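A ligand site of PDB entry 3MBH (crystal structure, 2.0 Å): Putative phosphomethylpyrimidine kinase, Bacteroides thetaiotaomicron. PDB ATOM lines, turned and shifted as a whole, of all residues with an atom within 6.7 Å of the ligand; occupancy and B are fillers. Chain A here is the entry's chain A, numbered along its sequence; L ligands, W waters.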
ATOM      1  N   HIS A  14      -9.248  -4.326  20.838  1.00  0.00           N
ATOM      2  CA  HIS A  14     -10.029  -3.900  21.943  1.00  0.00           C
ATOM      3  C   HIS A  14     -10.957  -2.811  21.442  1.00  0.00           C
ATOM      4  O   HIS A  14     -10.732  -2.231  20.381  1.00  0.00           O
ATOM      5  CB  HIS A  14      -9.165  -3.267  23.054  1.00  0.00           C
ATOM      6  CG  HIS A  14      -8.157  -4.186  23.666  1.00  0.00           C
ATOM      7  ND1 HIS A  14      -8.344  -4.759  24.900  1.00  0.00           N
ATOM      8  CD2 HIS A  14      -6.915  -4.564  23.265  1.00  0.00           C
ATOM      9  CE1 HIS A  14      -7.301  -5.519  25.205  1.00  0.00           C
ATOM     10  NE2 HIS A  14      -6.419  -5.422  24.224  1.00  0.00           N
ATOM     11  N   ASP A  15     -11.990  -2.528  22.221  1.00  0.00           N
ATOM     12  CA  ASP A  15     -12.862  -1.422  21.968  1.00  0.00           C
ATOM     13  C   ASP A  15     -12.272  -0.046  22.343  1.00  0.00           C
ATOM     14  O   ASP A  15     -11.269   0.072  23.074  1.00  0.00           O
ATOM     15  CB  ASP A  15     -14.167  -1.664  22.676  1.00  0.00           C
ATOM     16  CG  ASP A  15     -14.029  -1.510  24.172  1.00  0.00           C
ATOM     17  OD1 ASP A  15     -13.738  -2.552  24.859  1.00  0.00           O
ATOM     18  OD2 ASP A  15     -14.110  -0.340  24.637  1.00  0.00           O
ATOM     19  N   LEU A  16     -12.885   1.011  21.800  1.00  0.00           N
ATOM     20  CA  LEU A  16     -12.607   2.396  22.156  1.00  0.00           C
ATOM     21  C   LEU A  16     -13.810   2.930  22.887  1.00  0.00           C
ATOM     22  O   LEU A  16     -14.888   3.068  22.295  1.00  0.00           O
ATOM     23  CB  LEU A  16     -12.324   3.254  20.946  1.00  0.00           C
ATOM     24  CG  LEU A  16     -11.799   4.713  21.200  1.00  0.00           C
ATOM     25  CD1 LEU A  16     -10.337   4.687  21.710  1.00  0.00           C
ATOM     26  CD2 LEU A  16     -11.884   5.574  19.984  1.00  0.00           C
ATOM     27  N   SER A  17     -13.599   3.190  24.181  1.00  0.00           N
ATOM     28  CA  SER A  17     -14.574   3.758  25.050  1.00  0.00           C
ATOM     29  C   SER A  17     -14.174   5.176  25.497  1.00  0.00           C
ATOM     30  O   SER A  17     -13.097   5.395  26.005  1.00  0.00           O
ATOM     31  CB  SER A  17     -14.751   2.902  26.310  1.00  0.00           C
ATOM     32  OG  SER A  17     -15.532   1.779  26.057  1.00  0.00           O
ATOM     33  N   VAL A  22     -11.004   1.659  30.423  1.00  0.00           N
ATOM     34  CA  VAL A  22     -11.053   0.296  29.944  1.00  0.00           C
ATOM     35  C   VAL A  22     -10.378   0.260  28.592  1.00  0.00           C
ATOM     36  O   VAL A  22     -10.114   1.291  27.977  1.00  0.00           O
ATOM     37  CB  VAL A  22     -12.492  -0.230  29.796  1.00  0.00           C
ATOM     38  CG1 VAL A  22     -13.184  -0.353  31.184  1.00  0.00           C
ATOM     39  CG2 VAL A  22     -13.325   0.639  28.782  1.00  0.00           C
ATOM     40  N   SER A  23     -10.067  -0.943  28.154  1.00  0.00           N
ATOM     41  CA  SER A  23      -9.803  -1.218  26.740  1.00  0.00           C
ATOM     42  C   SER A  23      -8.732  -0.275  26.126  1.00  0.00           C
ATOM     43  O   SER A  23      -7.673  -0.064  26.739  1.00  0.00           O
ATOM     44  CB  SER A  23     -11.115  -1.269  25.963  1.00  0.00           C
ATOM     45  OG  SER A  23     -11.859  -0.061  26.047  1.00  0.00           O
ATOM     46  N   ALA A  44     -15.231  -2.008  18.627  1.00  0.00           N
ATOM     47  CA  ALA A  44     -16.471  -1.305  18.914  1.00  0.00           C
ATOM     48  C   ALA A  44     -16.123   0.112  19.336  1.00  0.00           C
ATOM     49  O   ALA A  44     -15.017   0.352  19.787  1.00  0.00           O
ATOM     50  CB  ALA A  44     -17.285  -1.981  20.037  1.00  0.00           C
ATOM     51  N   LEU A  46     -17.740   2.976  22.002  1.00  0.00           N
ATOM     52  CA  LEU A  46     -18.712   3.250  23.057  1.00  0.00           C
ATOM     53  C   LEU A  46     -18.445   4.607  23.691  1.00  0.00           C
ATOM     54  O   LEU A  46     -17.302   5.026  23.813  1.00  0.00           O
ATOM     55  CB  LEU A  46     -18.657   2.140  24.142  1.00  0.00           C
ATOM     56  CG  LEU A  46     -18.868   0.649  23.760  1.00  0.00           C
ATOM     57  CD1 LEU A  46     -17.594  -0.039  23.227  1.00  0.00           C
ATOM     58  CD2 LEU A  46     -19.380  -0.155  24.994  1.00  0.00           C
ATOM     59  N   ASN A  48     -18.764   5.025  26.830  1.00  0.00           N
ATOM     60  CA  ASN A  48     -18.256   4.651  28.134  1.00  0.00           C
ATOM     61  C   ASN A  48     -18.401   3.151  28.324  1.00  0.00           C
ATOM     62  O   ASN A  48     -19.156   2.513  27.596  1.00  0.00           O
ATOM     63  CB  ASN A  48     -19.023   5.384  29.238  1.00  0.00           C
ATOM     64  CG  ASN A  48     -20.547   5.284  29.115  1.00  0.00           C
ATOM     65  OD1 ASN A  48     -21.210   6.207  28.615  1.00  0.00           O
ATOM     66  ND2 ASN A  48     -21.111   4.188  29.619  1.00  0.00           N
ATOM     67  N   HIS A  49     -17.761   2.599  29.355  1.00  0.00           N
ATOM     68  CA  HIS A  49     -17.825   1.148  29.521  1.00  0.00           C
ATOM     69  C   HIS A  49     -19.238   0.689  29.899  1.00  0.00           C
ATOM     70  O   HIS A  49     -20.112   1.515  30.261  1.00  0.00           O
ATOM     71  CB  HIS A  49     -16.741   0.615  30.498  1.00  0.00           C
ATOM     72  CG  HIS A  49     -16.877   1.120  31.905  1.00  0.00           C
ATOM     73  ND1 HIS A  49     -17.989   0.904  32.680  1.00  0.00           N
ATOM     74  CD2 HIS A  49     -16.026   1.854  32.666  1.00  0.00           C
ATOM     75  CE1 HIS A  49     -17.817   1.470  33.861  1.00  0.00           C
ATOM     76  NE2 HIS A  49     -16.636   2.073  33.872  1.00  0.00           N
ATOM     77  N   THR A  50     -19.472  -0.621  29.781  1.00  0.00           N
ATOM     78  CA  THR A  50     -20.807  -1.203  29.978  1.00  0.00           C
ATOM     79  C   THR A  50     -21.213  -1.486  31.436  1.00  0.00           C
ATOM     80  O   THR A  50     -22.269  -2.072  31.695  1.00  0.00           O
ATOM     81  CB  THR A  50     -20.954  -2.489  29.147  1.00  0.00           C
ATOM     82  OG1 THR A  50     -20.028  -3.467  29.616  1.00  0.00           O
ATOM     83  CG2 THR A  50     -20.728  -2.196  27.671  1.00  0.00           C
ATOM     84  N   GLN A  51     -20.405  -1.072  32.400  1.00  0.00           N
ATOM     85  CA  GLN A  51     -20.798  -1.142  33.818  1.00  0.00           C
ATOM     86  C   GLN A  51     -21.415   0.178  34.319  1.00  0.00           C
ATOM     87  O   GLN A  51     -21.837   0.295  35.459  1.00  0.00           O
ATOM     88  CB  GLN A  51     -19.630  -1.604  34.676  1.00  0.00           C
ATOM     89  CG  GLN A  51     -19.057  -2.981  34.255  1.00  0.00           C
ATOM     90  CD  GLN A  51     -18.031  -3.532  35.237  1.00  0.00           C
ATOM     91  OE1 GLN A  51     -18.347  -3.708  36.417  1.00  0.00           O
ATOM     92  NE2 GLN A  51     -16.824  -3.870  34.751  1.00  0.00           N
ATOM     93  N   PHE A  57     -23.254   2.349  21.656  1.00  0.00           N
ATOM     94  CA  PHE A  57     -22.538   1.199  21.188  1.00  0.00           C
ATOM     95  C   PHE A  57     -22.569   1.134  19.650  1.00  0.00           C
ATOM     96  O   PHE A  57     -23.622   1.136  19.042  1.00  0.00           O
ATOM     97  CB  PHE A  57     -23.164  -0.066  21.774  1.00  0.00           C
ATOM     98  CG  PHE A  57     -22.434  -1.301  21.417  1.00  0.00           C
ATOM     99  CD1 PHE A  57     -21.304  -1.656  22.106  1.00  0.00           C
ATOM    100  CD2 PHE A  57     -22.822  -2.070  20.320  1.00  0.00           C
ATOM    101  CE1 PHE A  57     -20.580  -2.781  21.775  1.00  0.00           C
ATOM    102  CE2 PHE A  57     -22.090  -3.203  19.973  1.00  0.00           C
ATOM    103  CZ  PHE A  57     -20.987  -3.570  20.704  1.00  0.00           C
ATOM    104  N   GLY A  84      -8.847  -8.145  23.708  1.00  0.00           N
ATOM    105  CA  GLY A  84      -9.729  -8.016  24.855  1.00  0.00           C
ATOM    106  C   GLY A  84     -11.203  -8.000  24.478  1.00  0.00           C
ATOM    107  O   GLY A  84     -11.745  -8.982  23.829  1.00  0.00           O
ATOM    108  N   TYR A  85     -11.888  -6.966  24.920  1.00  0.00           N
ATOM    109  CA  TYR A  85     -13.317  -6.852  24.674  1.00  0.00           C
ATOM    110  C   TYR A  85     -13.599  -6.847  23.164  1.00  0.00           C
ATOM    111  O   TYR A  85     -13.118  -6.021  22.453  1.00  0.00           O
ATOM    112  CB  TYR A  85     -13.850  -5.585  25.351  1.00  0.00           C
ATOM    113  CG  TYR A  85     -15.352  -5.373  25.312  1.00  0.00           C
ATOM    114  CD1 TYR A  85     -15.977  -4.954  24.136  1.00  0.00           C
ATOM    115  CD2 TYR A  85     -16.169  -5.615  26.434  1.00  0.00           C
ATOM    116  CE1 TYR A  85     -17.343  -4.762  24.074  1.00  0.00           C
ATOM    117  CE2 TYR A  85     -17.521  -5.395  26.376  1.00  0.00           C
ATOM    118  CZ  TYR A  85     -18.104  -4.986  25.177  1.00  0.00           C
ATOM    119  OH  TYR A  85     -19.456  -4.757  25.091  1.00  0.00           O
ATOM    120  N   ASP A 112      -6.963 -11.558  26.660  1.00  0.00           N
ATOM    121  CA  ASP A 112      -7.764 -11.397  27.841  1.00  0.00           C
ATOM    122  C   ASP A 112      -9.188 -11.829  27.447  1.00  0.00           C
ATOM    123  O   ASP A 112      -9.803 -11.221  26.594  1.00  0.00           O
ATOM    124  CB  ASP A 112      -7.682  -9.918  28.338  1.00  0.00           C
ATOM    125  CG  ASP A 112      -8.482  -9.682  29.615  1.00  0.00           C
ATOM    126  OD1 ASP A 112      -9.273 -10.588  30.038  1.00  0.00           O
ATOM    127  OD2 ASP A 112      -8.341  -8.563  30.212  1.00  0.00           O
ATOM    128  N   VAL A 114     -12.298 -11.388  27.820  1.00  0.00           N
ATOM    129  CA  VAL A 114     -13.226 -10.412  28.409  1.00  0.00           C
ATOM    130  C   VAL A 114     -14.681 -10.883  28.201  1.00  0.00           C
ATOM    131  O   VAL A 114     -15.215 -10.858  27.074  1.00  0.00           O
ATOM    132  CB  VAL A 114     -12.976  -8.993  27.860  1.00  0.00           C
ATOM    133  CG1 VAL A 114     -13.981  -7.916  28.483  1.00  0.00           C
ATOM    134  CG2 VAL A 114     -11.491  -8.541  28.104  1.00  0.00           C
ATOM    135  N   TYR A 122     -20.866  -9.522  31.192  1.00  0.00           N
ATOM    136  CA  TYR A 122     -21.081  -8.099  30.920  1.00  0.00           C
ATOM    137  C   TYR A 122     -22.336  -7.837  30.060  1.00  0.00           C
ATOM    138  O   TYR A 122     -22.838  -8.721  29.333  1.00  0.00           O
ATOM    139  CB  TYR A 122     -19.878  -7.472  30.224  1.00  0.00           C
ATOM    140  CG  TYR A 122     -18.621  -7.424  31.049  1.00  0.00           C
ATOM    141  CD1 TYR A 122     -18.637  -6.972  32.370  1.00  0.00           C
ATOM    142  CD2 TYR A 122     -17.430  -7.870  30.513  1.00  0.00           C
ATOM    143  CE1 TYR A 122     -17.456  -6.902  33.112  1.00  0.00           C
ATOM    144  CE2 TYR A 122     -16.232  -7.850  31.263  1.00  0.00           C
ATOM    145  CZ  TYR A 122     -16.255  -7.336  32.537  1.00  0.00           C
ATOM    146  OH  TYR A 122     -15.102  -7.324  33.247  1.00  0.00           O
ATOM    147  N   THR A 123     -22.848  -6.609  30.122  1.00  0.00           N
ATOM    148  CA  THR A 123     -24.178  -6.298  29.556  1.00  0.00           C
ATOM    149  C   THR A 123     -24.215  -6.679  28.089  1.00  0.00           C
ATOM    150  O   THR A 123     -23.281  -6.326  27.307  1.00  0.00           O
ATOM    151  CB  THR A 123     -24.484  -4.788  29.683  1.00  0.00           C
ATOM    152  OG1 THR A 123     -24.442  -4.447  31.074  1.00  0.00           O
ATOM    153  CG2 THR A 123     -25.856  -4.409  29.098  1.00  0.00           C
ATOM    154  N   GLU A 149     -14.682 -15.407  34.434  1.00  0.00           N
ATOM    155  CA  GLU A 149     -14.363 -15.792  33.077  1.00  0.00           C
ATOM    156  C   GLU A 149     -13.787 -17.205  33.053  1.00  0.00           C
ATOM    157  O   GLU A 149     -14.065 -17.970  32.128  1.00  0.00           O
ATOM    158  CB  GLU A 149     -13.412 -14.769  32.463  1.00  0.00           C
ATOM    159  CG  GLU A 149     -14.077 -13.462  32.243  1.00  0.00           C
ATOM    160  CD  GLU A 149     -13.151 -12.282  32.074  1.00  0.00           C
ATOM    161  OE1 GLU A 149     -11.928 -12.353  32.397  1.00  0.00           O
ATOM    162  OE2 GLU A 149     -13.680 -11.271  31.569  1.00  0.00           O
ATOM    163  N   PRO A 221     -13.764  -0.987  37.248  1.00  0.00           N
ATOM    164  CA  PRO A 221     -13.884  -1.488  35.912  1.00  0.00           C
ATOM    165  C   PRO A 221     -12.627  -1.169  35.130  1.00  0.00           C
ATOM    166  O   PRO A 221     -12.045  -0.091  35.323  1.00  0.00           O
ATOM    167  CB  PRO A 221     -15.057  -0.700  35.361  1.00  0.00           C
ATOM    168  CG  PRO A 221     -15.907  -0.496  36.583  1.00  0.00           C
ATOM    169  CD  PRO A 221     -14.854  -0.043  37.545  1.00  0.00           C
ATOM    170  N   GLY A 222     -12.208  -2.150  34.327  1.00  0.00           N
ATOM    171  CA  GLY A 222     -11.048  -2.058  33.480  1.00  0.00           C
ATOM    172  C   GLY A 222      -9.737  -2.442  34.136  1.00  0.00           C
ATOM    173  O   GLY A 222      -8.699  -2.311  33.527  1.00  0.00           O
ATOM    174  N   THR A 223      -9.779  -2.908  35.384  1.00  0.00           N
ATOM    175  CA  THR A 223      -8.533  -3.322  36.024  1.00  0.00           C
ATOM    176  C   THR A 223      -7.905  -4.558  35.364  1.00  0.00           C
ATOM    177  O   THR A 223      -6.694  -4.734  35.418  1.00  0.00           O
ATOM    178  CB  THR A 223      -8.753  -3.594  37.492  1.00  0.00           C
ATOM    179  OG1 THR A 223      -9.125  -2.364  38.154  1.00  0.00           O
ATOM    180  CG2 THR A 223      -7.492  -4.184  38.131  1.00  0.00           C
ATOM    181  N   GLY A 224      -8.727  -5.398  34.730  1.00  0.00           N
ATOM    182  CA  GLY A 224      -8.211  -6.494  33.910  1.00  0.00           C
ATOM    183  C   GLY A 224      -7.425  -6.015  32.679  1.00  0.00           C
ATOM    184  O   GLY A 224      -6.448  -6.621  32.279  1.00  0.00           O
ATOM    185  N   ASP A 225      -7.861  -4.898  32.091  1.00  0.00           N
ATOM    186  CA  ASP A 225      -7.161  -4.306  31.006  1.00  0.00           C
ATOM    187  C   ASP A 225      -5.838  -3.699  31.471  1.00  0.00           C
ATOM    188  O   ASP A 225      -4.817  -3.831  30.793  1.00  0.00           O
ATOM    189  CB  ASP A 225      -8.019  -3.266  30.270  1.00  0.00           C
ATOM    190  CG  ASP A 225      -9.325  -3.861  29.721  1.00  0.00           C
ATOM    191  OD1 ASP A 225      -9.322  -4.975  29.130  1.00  0.00           O
ATOM    192  OD2 ASP A 225     -10.357  -3.176  29.933  1.00  0.00           O
HETATM  193  O1  LIG L   1     -12.079  -5.173  29.688  1.00  0.00           O
HETATM  194  C1  LIG L   1     -13.173  -4.624  30.402  1.00  0.00           C
HETATM  195  C2  LIG L   1     -14.075  -3.863  29.421  1.00  0.00           C
HETATM  196  C3  LIG L   1     -13.707  -3.447  28.158  1.00  0.00           C
HETATM  197  N1  LIG L   1     -14.562  -2.827  27.343  1.00  0.00           N
HETATM  198  C4  LIG L   1     -15.823  -2.474  27.639  1.00  0.00           C
HETATM  199  C5  LIG L   1     -16.323  -2.843  28.962  1.00  0.00           C
HETATM  200  C6  LIG L   1     -15.410  -3.587  29.854  1.00  0.00           C
HETATM  201  C7  LIG L   1     -15.735  -3.983  31.226  1.00  0.00           C
HETATM  202  O2  LIG L   1     -16.704  -3.432  31.644  1.00  0.00           O
HETATM  203  O3  LIG L   1     -17.577  -2.617  29.398  1.00  0.00           O
HETATM  204  C8  LIG L   1     -16.587  -1.707  26.563  1.00  0.00           C
HETATM  205  O   HOH W   1     -10.618  -4.804  26.668  1.00  0.00           O
HETATM  206  O   HOH W   2     -10.553  -7.077  31.200  1.00  0.00           O
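N of Thr 50 is in hydrogen-bond range of O3 of the ligand, at 2.8 Å.
NE2 of Gln 51 sits at hydrogen-bond distance from O2 of the ligand.
The side-chain hydroxyl of Thr 50 sits at hydrogen-bond distance from an oxygen (O3) of the ligand, 2.6 Å away.
The side-chain carboxylate of Asp 15 lies within hydrogen-bond range of a nitrogen (N1) of the ligand.
The side-chain carboxylate (OD2) of Asp 225 sits at hydrogen-bond distance from an oxygen (O1) of the ligand (2.6 Å).
The backbone NH of Leu 46 is in hydrogen-bond range of the backbone carbonyl oxygen of Leu 16, 2.9 Å away.
N of Gln 51 is in hydrogen-bond range of ND1 of His 49 (3.1 Å).
The side-chain carboxylate of Asp 225 lies within hydrogen-bond range of the backbone NH of Ser 23 (2.9 Å).
The side-chain hydroxyl of Ser 17 is in hydrogen-bond range of the side-chain carboxylate of Asp 15 (2.9 Å).
The side-chain hydroxyl of Ser 23 is in hydrogen-bond range of the side-chain carboxylate of Asp 15 (2.7 Å).
O of Thr 50 is in hydrogen-bond range of OG1 of Thr 123.
Merely in contact with the ligand: Tyr 85, His 49, Val 114, Leu 46, Tyr 122, Ser 17 and Val 22.
Hydrophobic or aromatic side chains that line the ligand: Val 22, Leu 46, His 49, Tyr 85, Val 114 and Tyr 122.
Of the 25 residues printed, 11 come within 4 Å of the ligand.
Water W2 lies within hydrogen-bond range of OD2 of Asp 112 (2.8 Å), O1 of the ligand (2.9 Å) and OD1 of Asp 225 (3.2 Å).
Water W1 lies within hydrogen-bond range of OD1 of Asp 225 (2.8 Å), ND1 of His 14 (2.9 Å), N of Tyr 85 (3.1 Å) and O1 of the ligand (3.4 Å).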
